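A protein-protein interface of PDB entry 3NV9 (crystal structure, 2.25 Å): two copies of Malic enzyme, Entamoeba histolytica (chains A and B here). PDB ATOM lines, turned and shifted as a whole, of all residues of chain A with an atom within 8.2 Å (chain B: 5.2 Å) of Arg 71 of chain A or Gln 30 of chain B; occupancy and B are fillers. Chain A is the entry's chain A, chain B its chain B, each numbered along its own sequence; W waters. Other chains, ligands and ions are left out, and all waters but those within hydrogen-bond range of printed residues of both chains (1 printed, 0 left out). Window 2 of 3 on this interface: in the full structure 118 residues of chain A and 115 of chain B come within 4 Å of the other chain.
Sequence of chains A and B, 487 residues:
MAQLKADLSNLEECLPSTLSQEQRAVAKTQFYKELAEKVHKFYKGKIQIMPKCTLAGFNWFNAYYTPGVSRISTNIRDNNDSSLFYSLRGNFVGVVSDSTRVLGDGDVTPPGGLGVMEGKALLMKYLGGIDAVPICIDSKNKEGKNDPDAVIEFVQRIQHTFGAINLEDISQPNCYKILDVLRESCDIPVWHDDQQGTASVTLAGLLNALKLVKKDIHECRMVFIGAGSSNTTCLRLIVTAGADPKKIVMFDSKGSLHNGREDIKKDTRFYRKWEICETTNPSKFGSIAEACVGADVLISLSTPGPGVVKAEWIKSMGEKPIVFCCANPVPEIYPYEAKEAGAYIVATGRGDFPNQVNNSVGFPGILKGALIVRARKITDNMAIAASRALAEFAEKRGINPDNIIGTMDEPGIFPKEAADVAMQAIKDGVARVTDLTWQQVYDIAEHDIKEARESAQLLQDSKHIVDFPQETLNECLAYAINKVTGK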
ATOM      1  N   ALA A  63     -19.271 -12.571 -14.874  1.00  0.00           N
ATOM      2  CA  ALA A  63     -20.619 -12.580 -14.315  1.00  0.00           C
ATOM      3  C   ALA A  63     -20.864 -11.420 -13.369  1.00  0.00           C
ATOM      4  O   ALA A  63     -21.997 -10.919 -13.225  1.00  0.00           O
ATOM      5  CB  ALA A  63     -20.899 -13.928 -13.583  1.00  0.00           C
ATOM      6  N   TYR A  65     -19.499  -8.478 -13.483  1.00  0.00           N
ATOM      7  CA  TYR A  65     -19.023  -7.239 -14.107  1.00  0.00           C
ATOM      8  C   TYR A  65     -19.386  -7.396 -15.598  1.00  0.00           C
ATOM      9  O   TYR A  65     -20.090  -8.325 -15.974  1.00  0.00           O
ATOM     10  CB  TYR A  65     -17.515  -7.168 -13.903  1.00  0.00           C
ATOM     11  CG  TYR A  65     -16.861  -5.837 -14.128  1.00  0.00           C
ATOM     12  CD1 TYR A  65     -17.255  -4.730 -13.414  1.00  0.00           C
ATOM     13  CD2 TYR A  65     -15.761  -5.717 -15.016  1.00  0.00           C
ATOM     14  CE1 TYR A  65     -16.641  -3.512 -13.598  1.00  0.00           C
ATOM     15  CE2 TYR A  65     -15.135  -4.503 -15.238  1.00  0.00           C
ATOM     16  CZ  TYR A  65     -15.599  -3.382 -14.513  1.00  0.00           C
ATOM     17  OH  TYR A  65     -14.994  -2.144 -14.635  1.00  0.00           O
ATOM     18  N   PRO A  67     -19.500  -8.643 -19.185  1.00  0.00           N
ATOM     19  CA  PRO A  67     -20.804  -8.269 -19.681  1.00  0.00           C
ATOM     20  C   PRO A  67     -21.979  -8.703 -18.830  1.00  0.00           C
ATOM     21  O   PRO A  67     -23.048  -8.046 -18.905  1.00  0.00           O
ATOM     22  CB  PRO A  67     -20.876  -8.986 -21.055  1.00  0.00           C
ATOM     23  CG  PRO A  67     -20.171 -10.257 -20.809  1.00  0.00           C
ATOM     24  CD  PRO A  67     -19.010  -9.871 -19.830  1.00  0.00           C
ATOM     25  N   GLY A  68     -21.837  -9.780 -18.047  1.00  0.00           N
ATOM     26  CA  GLY A  68     -23.008 -10.309 -17.283  1.00  0.00           C
ATOM     27  C   GLY A  68     -23.785  -9.293 -16.438  1.00  0.00           C
ATOM     28  O   GLY A  68     -25.007  -9.345 -16.377  1.00  0.00           O
ATOM     29  N   VAL A  69     -23.094  -8.361 -15.775  1.00  0.00           N
ATOM     30  CA  VAL A  69     -23.752  -7.502 -14.787  1.00  0.00           C
ATOM     31  C   VAL A  69     -24.903  -6.679 -15.373  1.00  0.00           C
ATOM     32  O   VAL A  69     -25.744  -6.136 -14.669  1.00  0.00           O
ATOM     33  CB  VAL A  69     -22.703  -6.572 -14.082  1.00  0.00           C
ATOM     34  CG1 VAL A  69     -22.208  -5.498 -15.007  1.00  0.00           C
ATOM     35  CG2 VAL A  69     -23.263  -5.978 -12.789  1.00  0.00           C
ATOM     36  N   SER A  70     -24.926  -6.572 -16.689  1.00  0.00           N
ATOM     37  CA  SER A  70     -25.968  -5.817 -17.407  1.00  0.00           C
ATOM     38  C   SER A  70     -27.352  -6.416 -17.166  1.00  0.00           C
ATOM     39  O   SER A  70     -28.317  -5.682 -17.028  1.00  0.00           O
ATOM     40  CB  SER A  70     -25.593  -5.744 -18.905  1.00  0.00           C
ATOM     41  OG  SER A  70     -26.737  -5.610 -19.706  1.00  0.00           O
ATOM     42  N   ARG A  71     -27.450  -7.740 -17.082  1.00  0.00           N
ATOM     43  CA  ARG A  71     -28.693  -8.404 -16.639  1.00  0.00           C
ATOM     44  C   ARG A  71     -29.189  -7.877 -15.310  1.00  0.00           C
ATOM     45  O   ARG A  71     -30.415  -7.695 -15.107  1.00  0.00           O
ATOM     46  CB  ARG A  71     -28.503  -9.936 -16.557  1.00  0.00           C
ATOM     47  CG  ARG A  71     -29.759 -10.712 -16.078  1.00  0.00           C
ATOM     48  CD  ARG A  71     -30.991 -10.587 -17.021  1.00  0.00           C
ATOM     49  NE  ARG A  71     -30.801 -11.357 -18.245  1.00  0.00           N
ATOM     50  CZ  ARG A  71     -30.878 -12.685 -18.286  1.00  0.00           C
ATOM     51  NH1 ARG A  71     -31.195 -13.376 -17.175  1.00  0.00           N
ATOM     52  NH2 ARG A  71     -30.659 -13.323 -19.432  1.00  0.00           N
ATOM     53  N   ILE A  72     -28.253  -7.617 -14.390  1.00  0.00           N
ATOM     54  CA  ILE A  72     -28.634  -7.058 -13.097  1.00  0.00           C
ATOM     55  C   ILE A  72     -29.141  -5.630 -13.261  1.00  0.00           C
ATOM     56  O   ILE A  72     -30.142  -5.256 -12.652  1.00  0.00           O
ATOM     57  CB  ILE A  72     -27.495  -7.111 -12.038  1.00  0.00           C
ATOM     58  CG1 ILE A  72     -26.995  -8.553 -11.749  1.00  0.00           C
ATOM     59  CG2 ILE A  72     -27.930  -6.445 -10.711  1.00  0.00           C
ATOM     60  CD1 ILE A  72     -28.075  -9.620 -11.574  1.00  0.00           C
ATOM     61  N   SER A  73     -28.475  -4.825 -14.076  1.00  0.00           N
ATOM     62  CA  SER A  73     -28.905  -3.454 -14.275  1.00  0.00           C
ATOM     63  C   SER A  73     -30.329  -3.392 -14.807  1.00  0.00           C
ATOM     64  O   SER A  73     -31.148  -2.623 -14.323  1.00  0.00           O
ATOM     65  CB  SER A  73     -27.965  -2.721 -15.240  1.00  0.00           C
ATOM     66  OG  SER A  73     -26.598  -2.915 -14.863  1.00  0.00           O
ATOM     67  N   THR A  74     -30.635  -4.213 -15.802  1.00  0.00           N
ATOM     68  CA  THR A  74     -31.964  -4.162 -16.426  1.00  0.00           C
ATOM     69  C   THR A  74     -33.018  -4.849 -15.533  1.00  0.00           C
ATOM     70  O   THR A  74     -34.158  -4.321 -15.365  1.00  0.00           O
ATOM     71  CB  THR A  74     -31.939  -4.675 -17.900  1.00  0.00           C
ATOM     72  OG1 THR A  74     -31.415  -6.000 -17.925  1.00  0.00           O
ATOM     73  CG2 THR A  74     -31.026  -3.753 -18.788  1.00  0.00           C
ATOM     74  N   ASN A  75     -32.631  -5.964 -14.908  1.00  0.00           N
ATOM     75  CA  ASN A  75     -33.515  -6.591 -13.899  1.00  0.00           C
ATOM     76  C   ASN A  75     -33.953  -5.609 -12.822  1.00  0.00           C
ATOM     77  O   ASN A  75     -35.151  -5.483 -12.515  1.00  0.00           O
ATOM     78  CB  ASN A  75     -32.858  -7.801 -13.246  1.00  0.00           C
ATOM     79  CG  ASN A  75     -32.882  -9.001 -14.120  1.00  0.00           C
ATOM     80  OD1 ASN A  75     -33.441  -8.962 -15.211  1.00  0.00           O
ATOM     81  ND2 ASN A  75     -32.284 -10.105 -13.648  1.00  0.00           N
ATOM     82  N   ILE A  76     -32.994  -4.887 -12.254  1.00  0.00           N
ATOM     83  CA  ILE A  76     -33.349  -3.897 -11.261  1.00  0.00           C
ATOM     84  C   ILE A  76     -34.238  -2.791 -11.860  1.00  0.00           C
ATOM     85  O   ILE A  76     -35.249  -2.452 -11.273  1.00  0.00           O
ATOM     86  CB  ILE A  76     -32.126  -3.304 -10.531  1.00  0.00           C
ATOM     87  CG1 ILE A  76     -31.379  -4.403  -9.779  1.00  0.00           C
ATOM     88  CG2 ILE A  76     -32.605  -2.311  -9.526  1.00  0.00           C
ATOM     89  CD1 ILE A  76     -30.197  -3.879  -8.923  1.00  0.00           C
ATOM     90  N   ARG A  77     -33.874  -2.240 -13.021  1.00  0.00           N
ATOM     91  CA  ARG A  77     -34.670  -1.140 -13.656  1.00  0.00           C
ATOM     92  C   ARG A  77     -36.152  -1.514 -13.732  1.00  0.00           C
ATOM     93  O   ARG A  77     -37.018  -0.745 -13.336  1.00  0.00           O
ATOM     94  CB  ARG A  77     -34.110  -0.855 -15.045  1.00  0.00           C
ATOM     95  CG  ARG A  77     -34.784   0.244 -15.848  1.00  0.00           C
ATOM     96  CD  ARG A  77     -35.350  -0.340 -17.116  1.00  0.00           C
ATOM     97  NE  ARG A  77     -34.355  -0.302 -18.174  1.00  0.00           N
ATOM     98  CZ  ARG A  77     -34.149  -1.237 -19.115  1.00  0.00           C
ATOM     99  NH1 ARG A  77     -34.830  -2.362 -19.153  1.00  0.00           N
ATOM    100  NH2 ARG A  77     -33.191  -1.038 -20.007  1.00  0.00           N
ATOM    101  N   ASP A  78     -36.415  -2.734 -14.201  1.00  0.00           N
ATOM    102  CA  ASP A  78     -37.775  -3.219 -14.434  1.00  0.00           C
ATOM    103  C   ASP A  78     -38.467  -3.832 -13.190  1.00  0.00           C
ATOM    104  O   ASP A  78     -39.679  -4.029 -13.176  1.00  0.00           O
ATOM    105  CB  ASP A  78     -37.802  -4.159 -15.673  1.00  0.00           C
ATOM    106  CG  ASP A  78     -37.299  -3.446 -16.939  1.00  0.00           C
ATOM    107  OD1 ASP A  78     -37.412  -2.211 -16.982  1.00  0.00           O
ATOM    108  OD2 ASP A  78     -36.766  -4.091 -17.868  1.00  0.00           O
ATOM    109  N   SER A  82     -36.300  -6.183  -6.761  1.00  0.00           N
ATOM    110  CA  SER A  82     -35.275  -7.179  -6.965  1.00  0.00           C
ATOM    111  C   SER A  82     -33.872  -6.642  -6.612  1.00  0.00           C
ATOM    112  O   SER A  82     -32.911  -7.438  -6.473  1.00  0.00           O
ATOM    113  CB  SER A  82     -35.290  -7.744  -8.391  1.00  0.00           C
ATOM    114  OG  SER A  82     -34.741  -6.819  -9.310  1.00  0.00           O
ATOM    115  N   TYR A  86     -30.496  -8.864  -5.581  1.00  0.00           N
ATOM    116  CA  TYR A  86     -29.460  -8.992  -6.608  1.00  0.00           C
ATOM    117  C   TYR A  86     -28.234  -8.252  -6.167  1.00  0.00           C
ATOM    118  O   TYR A  86     -27.244  -8.237  -6.891  1.00  0.00           O
ATOM    119  CB  TYR A  86     -29.881  -8.464  -7.984  1.00  0.00           C
ATOM    120  CG  TYR A  86     -30.753  -9.399  -8.724  1.00  0.00           C
ATOM    121  CD1 TYR A  86     -30.355 -10.713  -8.982  1.00  0.00           C
ATOM    122  CD2 TYR A  86     -31.974  -8.974  -9.202  1.00  0.00           C
ATOM    123  CE1 TYR A  86     -31.193 -11.574  -9.685  1.00  0.00           C
ATOM    124  CE2 TYR A  86     -32.810  -9.811  -9.878  1.00  0.00           C
ATOM    125  CZ  TYR A  86     -32.429 -11.114 -10.125  1.00  0.00           C
ATOM    126  OH  TYR A  86     -33.318 -11.922 -10.804  1.00  0.00           O
ATOM    127  N   VAL B  26     -22.558 -14.597 -29.142  1.00  0.00           N
ATOM    128  CA  VAL B  26     -23.857 -14.248 -28.558  1.00  0.00           C
ATOM    129  C   VAL B  26     -24.185 -15.175 -27.384  1.00  0.00           C
ATOM    130  O   VAL B  26     -24.741 -14.740 -26.380  1.00  0.00           O
ATOM    131  CB  VAL B  26     -24.996 -14.315 -29.635  1.00  0.00           C
ATOM    132  CG1 VAL B  26     -26.403 -14.242 -28.973  1.00  0.00           C
ATOM    133  CG2 VAL B  26     -24.790 -13.195 -30.705  1.00  0.00           C
ATOM    134  N   ALA B  27     -23.847 -16.450 -27.534  1.00  0.00           N
ATOM    135  CA  ALA B  27     -23.946 -17.422 -26.448  1.00  0.00           C
ATOM    136  C   ALA B  27     -23.085 -17.004 -25.248  1.00  0.00           C
ATOM    137  O   ALA B  27     -23.555 -17.030 -24.130  1.00  0.00           O
ATOM    138  CB  ALA B  27     -23.572 -18.812 -26.913  1.00  0.00           C
ATOM    139  N   LYS B  28     -21.823 -16.662 -25.470  1.00  0.00           N
ATOM    140  CA  LYS B  28     -21.024 -16.123 -24.383  1.00  0.00           C
ATOM    141  C   LYS B  28     -21.755 -14.994 -23.655  1.00  0.00           C
ATOM    142  O   LYS B  28     -21.893 -15.020 -22.412  1.00  0.00           O
ATOM    143  CB  LYS B  28     -19.668 -15.661 -24.902  1.00  0.00           C
ATOM    144  CG  LYS B  28     -18.676 -16.838 -25.060  1.00  0.00           C
ATOM    145  CD  LYS B  28     -17.549 -16.503 -26.034  1.00  0.00           C
ATOM    146  CE  LYS B  28     -16.724 -15.390 -25.515  1.00  0.00           C
ATOM    147  NZ  LYS B  28     -15.433 -15.424 -26.211  1.00  0.00           N
ATOM    148  N   THR B  29     -22.267 -14.017 -24.397  1.00  0.00           N
ATOM    149  CA  THR B  29     -22.923 -12.921 -23.698  1.00  0.00           C
ATOM    150  C   THR B  29     -24.219 -13.327 -22.960  1.00  0.00           C
ATOM    151  O   THR B  29     -24.469 -12.861 -21.871  1.00  0.00           O
ATOM    152  CB  THR B  29     -22.961 -11.570 -24.540  1.00  0.00           C
ATOM    153  OG1 THR B  29     -24.239 -10.905 -24.463  1.00  0.00           O
ATOM    154  CG2 THR B  29     -22.549 -11.786 -25.924  1.00  0.00           C
ATOM    155  N   GLN B  30     -24.998 -14.247 -23.521  1.00  0.00           N
ATOM    156  CA  GLN B  30     -26.192 -14.801 -22.843  1.00  0.00           C
ATOM    157  C   GLN B  30     -25.853 -15.672 -21.615  1.00  0.00           C
ATOM    158  O   GLN B  30     -26.489 -15.548 -20.573  1.00  0.00           O
ATOM    159  CB  GLN B  30     -27.061 -15.617 -23.824  1.00  0.00           C
ATOM    160  CG  GLN B  30     -27.879 -14.778 -24.823  1.00  0.00           C
ATOM    161  CD  GLN B  30     -28.633 -13.656 -24.158  1.00  0.00           C
ATOM    162  OE1 GLN B  30     -28.439 -12.503 -24.508  1.00  0.00           O
ATOM    163  NE2 GLN B  30     -29.455 -13.970 -23.171  1.00  0.00           N
ATOM    164  N   PHE B  31     -24.867 -16.548 -21.733  1.00  0.00           N
ATOM    165  CA  PHE B  31     -24.391 -17.278 -20.564  1.00  0.00           C
ATOM    166  C   PHE B  31     -24.098 -16.326 -19.383  1.00  0.00           C
ATOM    167  O   PHE B  31     -24.759 -16.381 -18.335  1.00  0.00           O
ATOM    168  CB  PHE B  31     -23.148 -18.086 -20.930  1.00  0.00           C
ATOM    169  CG  PHE B  31     -22.510 -18.770 -19.759  1.00  0.00           C
ATOM    170  CD1 PHE B  31     -23.112 -19.884 -19.182  1.00  0.00           C
ATOM    171  CD2 PHE B  31     -21.299 -18.292 -19.227  1.00  0.00           C
ATOM    172  CE1 PHE B  31     -22.523 -20.499 -18.114  1.00  0.00           C
ATOM    173  CE2 PHE B  31     -20.716 -18.911 -18.184  1.00  0.00           C
ATOM    174  CZ  PHE B  31     -21.319 -20.012 -17.611  1.00  0.00           C
ATOM    175  N   TYR B  32     -23.167 -15.393 -19.576  1.00  0.00           N
ATOM    176  CA  TYR B  32     -22.840 -14.473 -18.484  1.00  0.00           C
ATOM    177  C   TYR B  32     -24.004 -13.633 -18.017  1.00  0.00           C
ATOM    178  O   TYR B  32     -24.077 -13.323 -16.838  1.00  0.00           O
ATOM    179  CB  TYR B  32     -21.623 -13.596 -18.811  1.00  0.00           C
ATOM    180  CG  TYR B  32     -20.363 -14.408 -18.840  1.00  0.00           C
ATOM    181  CD1 TYR B  32     -19.946 -15.102 -17.723  1.00  0.00           C
ATOM    182  CD2 TYR B  32     -19.592 -14.488 -19.991  1.00  0.00           C
ATOM    183  CE1 TYR B  32     -18.792 -15.876 -17.749  1.00  0.00           C
ATOM    184  CE2 TYR B  32     -18.444 -15.232 -20.029  1.00  0.00           C
ATOM    185  CZ  TYR B  32     -18.045 -15.921 -18.901  1.00  0.00           C
ATOM    186  OH  TYR B  32     -16.897 -16.645 -18.919  1.00  0.00           O
ATOM    187  N   LYS B  33     -24.936 -13.276 -18.903  1.00  0.00           N
ATOM    188  CA  LYS B  33     -26.119 -12.564 -18.419  1.00  0.00           C
ATOM    189  C   LYS B  33     -26.988 -13.450 -17.504  1.00  0.00           C
ATOM    190  O   LYS B  33     -27.383 -13.045 -16.407  1.00  0.00           O
ATOM    191  CB  LYS B  33     -26.915 -11.997 -19.570  1.00  0.00           C
ATOM    192  CG  LYS B  33     -26.209 -10.799 -20.232  1.00  0.00           C
ATOM    193  CD  LYS B  33     -27.019 -10.216 -21.393  1.00  0.00           C
ATOM    194  CE  LYS B  33     -26.640  -8.731 -21.594  1.00  0.00           C
ATOM    195  NZ  LYS B  33     -27.143  -8.237 -22.874  1.00  0.00           N
ATOM    196  N   GLU B  34     -27.251 -14.670 -17.943  1.00  0.00           N
ATOM    197  CA  GLU B  34     -28.065 -15.599 -17.159  1.00  0.00           C
ATOM    198  C   GLU B  34     -27.326 -16.011 -15.879  1.00  0.00           C
ATOM    199  O   GLU B  34     -27.924 -16.035 -14.808  1.00  0.00           O
ATOM    200  CB  GLU B  34     -28.368 -16.831 -18.005  1.00  0.00           C
ATOM    201  CG  GLU B  34     -29.357 -17.800 -17.405  1.00  0.00           C
ATOM    202  CD  GLU B  34     -30.736 -17.186 -17.250  1.00  0.00           C
ATOM    203  OE1 GLU B  34     -30.985 -16.056 -17.780  1.00  0.00           O
ATOM    204  OE2 GLU B  34     -31.583 -17.849 -16.600  1.00  0.00           O
ATOM    205  N   LEU B  35     -26.036 -16.348 -15.993  1.00  0.00           N
ATOM    206  CA  LEU B  35     -25.197 -16.606 -14.796  1.00  0.00           C
ATOM    207  C   LEU B  35     -25.120 -15.443 -13.770  1.00  0.00           C
ATOM    208  O   LEU B  35     -25.253 -15.666 -12.572  1.00  0.00           O
ATOM    209  CB  LEU B  35     -23.789 -17.050 -15.181  1.00  0.00           C
ATOM    210  CG  LEU B  35     -22.888 -17.371 -13.980  1.00  0.00           C
ATOM    211  CD1 LEU B  35     -23.424 -18.542 -13.127  1.00  0.00           C
ATOM    212  CD2 LEU B  35     -21.504 -17.649 -14.510  1.00  0.00           C
ATOM    213  N   ALA B  36     -24.926 -14.216 -14.238  1.00  0.00           N
ATOM    214  CA  ALA B  36     -25.035 -13.046 -13.373  1.00  0.00           C
ATOM    215  C   ALA B  36     -26.351 -13.066 -12.606  1.00  0.00           C
ATOM    216  O   ALA B  36     -26.411 -12.820 -11.391  1.00  0.00           O
ATOM    217  CB  ALA B  36     -24.936 -11.747 -14.244  1.00  0.00           C
ATOM    218  N   GLU B  37     -27.445 -13.328 -13.319  1.00  0.00           N
ATOM    219  CA  GLU B  37     -28.737 -13.390 -12.647  1.00  0.00           C
ATOM    220  C   GLU B  37     -28.688 -14.416 -11.512  1.00  0.00           C
ATOM    221  O   GLU B  37     -29.054 -14.128 -10.363  1.00  0.00           O
ATOM    222  CB  GLU B  37     -29.858 -13.665 -13.650  1.00  0.00           C
ATOM    223  CG  GLU B  37     -31.236 -13.782 -13.002  1.00  0.00           C
ATOM    224  CD  GLU B  37     -32.380 -13.608 -13.963  1.00  0.00           C
ATOM    225  OE1 GLU B  37     -32.403 -12.655 -14.803  1.00  0.00           O
ATOM    226  OE2 GLU B  37     -33.285 -14.441 -13.859  1.00  0.00           O
ATOM    227  N   TYR B 479     -29.234 -22.823 -21.248  1.00  0.00           N
ATOM    228  CA  TYR B 479     -29.929 -21.609 -21.553  1.00  0.00           C
ATOM    229  C   TYR B 479     -29.219 -20.862 -22.702  1.00  0.00           C
ATOM    230  O   TYR B 479     -29.858 -20.513 -23.695  1.00  0.00           O
ATOM    231  CB  TYR B 479     -30.066 -20.741 -20.310  1.00  0.00           C
ATOM    232  CG  TYR B 479     -30.579 -19.326 -20.572  1.00  0.00           C
ATOM    233  CD1 TYR B 479     -31.954 -18.988 -20.421  1.00  0.00           C
ATOM    234  CD2 TYR B 479     -29.688 -18.314 -20.971  1.00  0.00           C
ATOM    235  CE1 TYR B 479     -32.389 -17.685 -20.687  1.00  0.00           C
ATOM    236  CE2 TYR B 479     -30.113 -17.041 -21.232  1.00  0.00           C
ATOM    237  CZ  TYR B 479     -31.424 -16.712 -21.072  1.00  0.00           C
ATOM    238  OH  TYR B 479     -31.751 -15.398 -21.346  1.00  0.00           O
ATOM    239  N   ALA B 480     -27.902 -20.666 -22.597  1.00  0.00           N
ATOM    240  CA  ALA B 480     -27.147 -19.884 -23.602  1.00  0.00           C
ATOM    241  C   ALA B 480     -27.159 -20.542 -24.992  1.00  0.00           C
ATOM    242  O   ALA B 480     -27.344 -19.845 -26.020  1.00  0.00           O
ATOM    243  CB  ALA B 480     -25.697 -19.674 -23.149  1.00  0.00           C
ATOM    244  N   LYS B 483     -30.571 -20.298 -26.708  1.00  0.00           N
ATOM    245  CA  LYS B 483     -30.863 -19.000 -27.295  1.00  0.00           C
ATOM    246  C   LYS B 483     -30.346 -18.790 -28.724  1.00  0.00           C
ATOM    247  O   LYS B 483     -30.941 -18.040 -29.487  1.00  0.00           O
ATOM    248  CB  LYS B 483     -30.378 -17.866 -26.390  1.00  0.00           C
ATOM    249  CG  LYS B 483     -31.285 -17.644 -25.191  1.00  0.00           C
ATOM    250  CD  LYS B 483     -31.553 -16.167 -24.943  1.00  0.00           C
ATOM    251  CE  LYS B 483     -32.954 -15.808 -25.318  1.00  0.00           C
ATOM    252  NZ  LYS B 483     -33.557 -15.057 -24.175  1.00  0.00           N
HETATM  253  O   HOH W   1     -34.910 -11.935 -15.825  1.00  0.00           O
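The guanidinium group of Arg 71 of chain A is in salt-bridge range of the side-chain carboxylate of Glu 34 of chain B.
The side-chain carboxylate of Glu 37 of chain B lies within salt-bridge range of the guanidinium group of Arg 71 of chain A, 2.8 Å away.
The guanidinium group (NH2) of Arg 71 of chain A lies within hydrogen-bond range of the side-chain hydroxyl (OH) of Tyr 479 of chain B (3.0 Å).
The side-chain amide nitrogen (ND2) of Asn 75 of chain A is in hydrogen-bond range of the side-chain carboxylate (OE1) of Glu 37 of chain B (2.8 Å).
Water W1 lies within hydrogen-bond range of OE1 of Glu 37 of chain B (2.8 Å) and OD1 of Asn 75 of chain A (3.4 Å).
The backbone carbonyl oxygen of Ser 70 of chain A sits at hydrogen-bond distance from the side-chain hydroxyl of Thr 74 of chain A (3.2 Å).
O of Arg 71 of chain A sits at hydrogen-bond distance from OG1 of Thr 74 of chain A (3.4 Å).
OD1 of Asn 75 of chain A lies close to O of Arg 71 of chain A (3.3 Å).
O of Asn 75 of chain A sits at hydrogen-bond distance from OG of Ser 82 of chain A (3.5 Å).
The side-chain amide nitrogen (NE2) of Gln 30 of chain B lies within hydrogen-bond range of the side-chain hydroxyl (OH) of Tyr 479 of chain B (3.3 Å).
OH of Tyr 479 of chain B sits at hydrogen-bond distance from NZ of Lys 483 of chain B, at 3.4 Å.
Printed residues of chain B within 4 Å of Ser 70 of chain A: Lys 33.
Of the printed residues of chain B, Arg 71 of chain A touches Gln 30 (3.98 Å), Lys 33 (3.3 Å), Glu 34 (2.8 Å), Glu 37 (2.8 Å) and Tyr 479 (3.0 Å).
Of the printed residues of chain A, Gln 30 of chain B touches Arg 71 (3.98 Å).
Printed residues of chain A within 4 Å of Lys 33 of chain B: Gly 68 (3.9 Å), Ser 70 (3.6 Å) and Arg 71 (3.3 Å).
Printed residues of chain A within 4 Å of Ala 36 of chain B: Ala 63 (3.2 Å), Gly 68 (3.2 Å) and Ile 72 (3.6 Å).
Printed residues of chain A within 4 Å of Glu 37 of chain B: Arg 71, Ile 72, Asn 75 and Tyr 86.
The nearest printed residue of chain A that does not touch Gln 30 of chain B is Pro 67 of chain A (6.8 Å).
The nearest printed residue of chain A that does not touch Glu 37 of chain B is Gly 68 of chain A (5.6 Å).
No position is printed for both chains.
Among the printed residues, merely in contact across the chains: Gly 68 of chain A with Ala 36 of chain B (3.2 Å), Ala 63 of chain A with Ala 36 of chain B (3.2 Å), Gly 68 of chain A with Tyr 32 of chain B (3.2 Å), Arg 71 of chain A with Lys 33 of chain B (3.3 Å), Tyr 86 of chain A with Glu 37 of chain B (3.4 Å), Ile 72 of chain A with Ala 36 of chain B (3.6 Å), Ser 70 of chain A with Lys 33 of chain B (3.6 Å), Ala 63 of chain A with Tyr 32 of chain B (3.9 Å), Ala 63 of chain A with Leu 35 of chain B (3.9 Å), Gly 68 of chain A with Lys 33 of chain B (3.9 Å), Ile 72 of chain A with Glu 37 of chain B (3.98 Å) and Arg 71 of chain A with Gln 30 of chain B (3.98 Å).
Of the 16 printed residues of chain A, 7 touch a printed residue of chain B.
Printed residues of chain A that touch a printed residue of chain B: Ala 63, Gly 68, Ser 70, Arg 71, Ile 72, Asn 75 and Tyr 86.
Hydrophobic or aromatic side chains of chain A that line the printed part of chain B: Ala 63, Ile 72 and Tyr 86.
Along chain B the printed residues that touch a printed residue of chain A span positions 30 to 479.
Among the printed residues, Asp or Glu carboxylates within 4 Å of a Lys or Arg side-chain nitrogen of the other chain: Arg 71 of chain A with Glu 34 of chain B and Arg 71 of chain A with Glu 37 of chain B.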
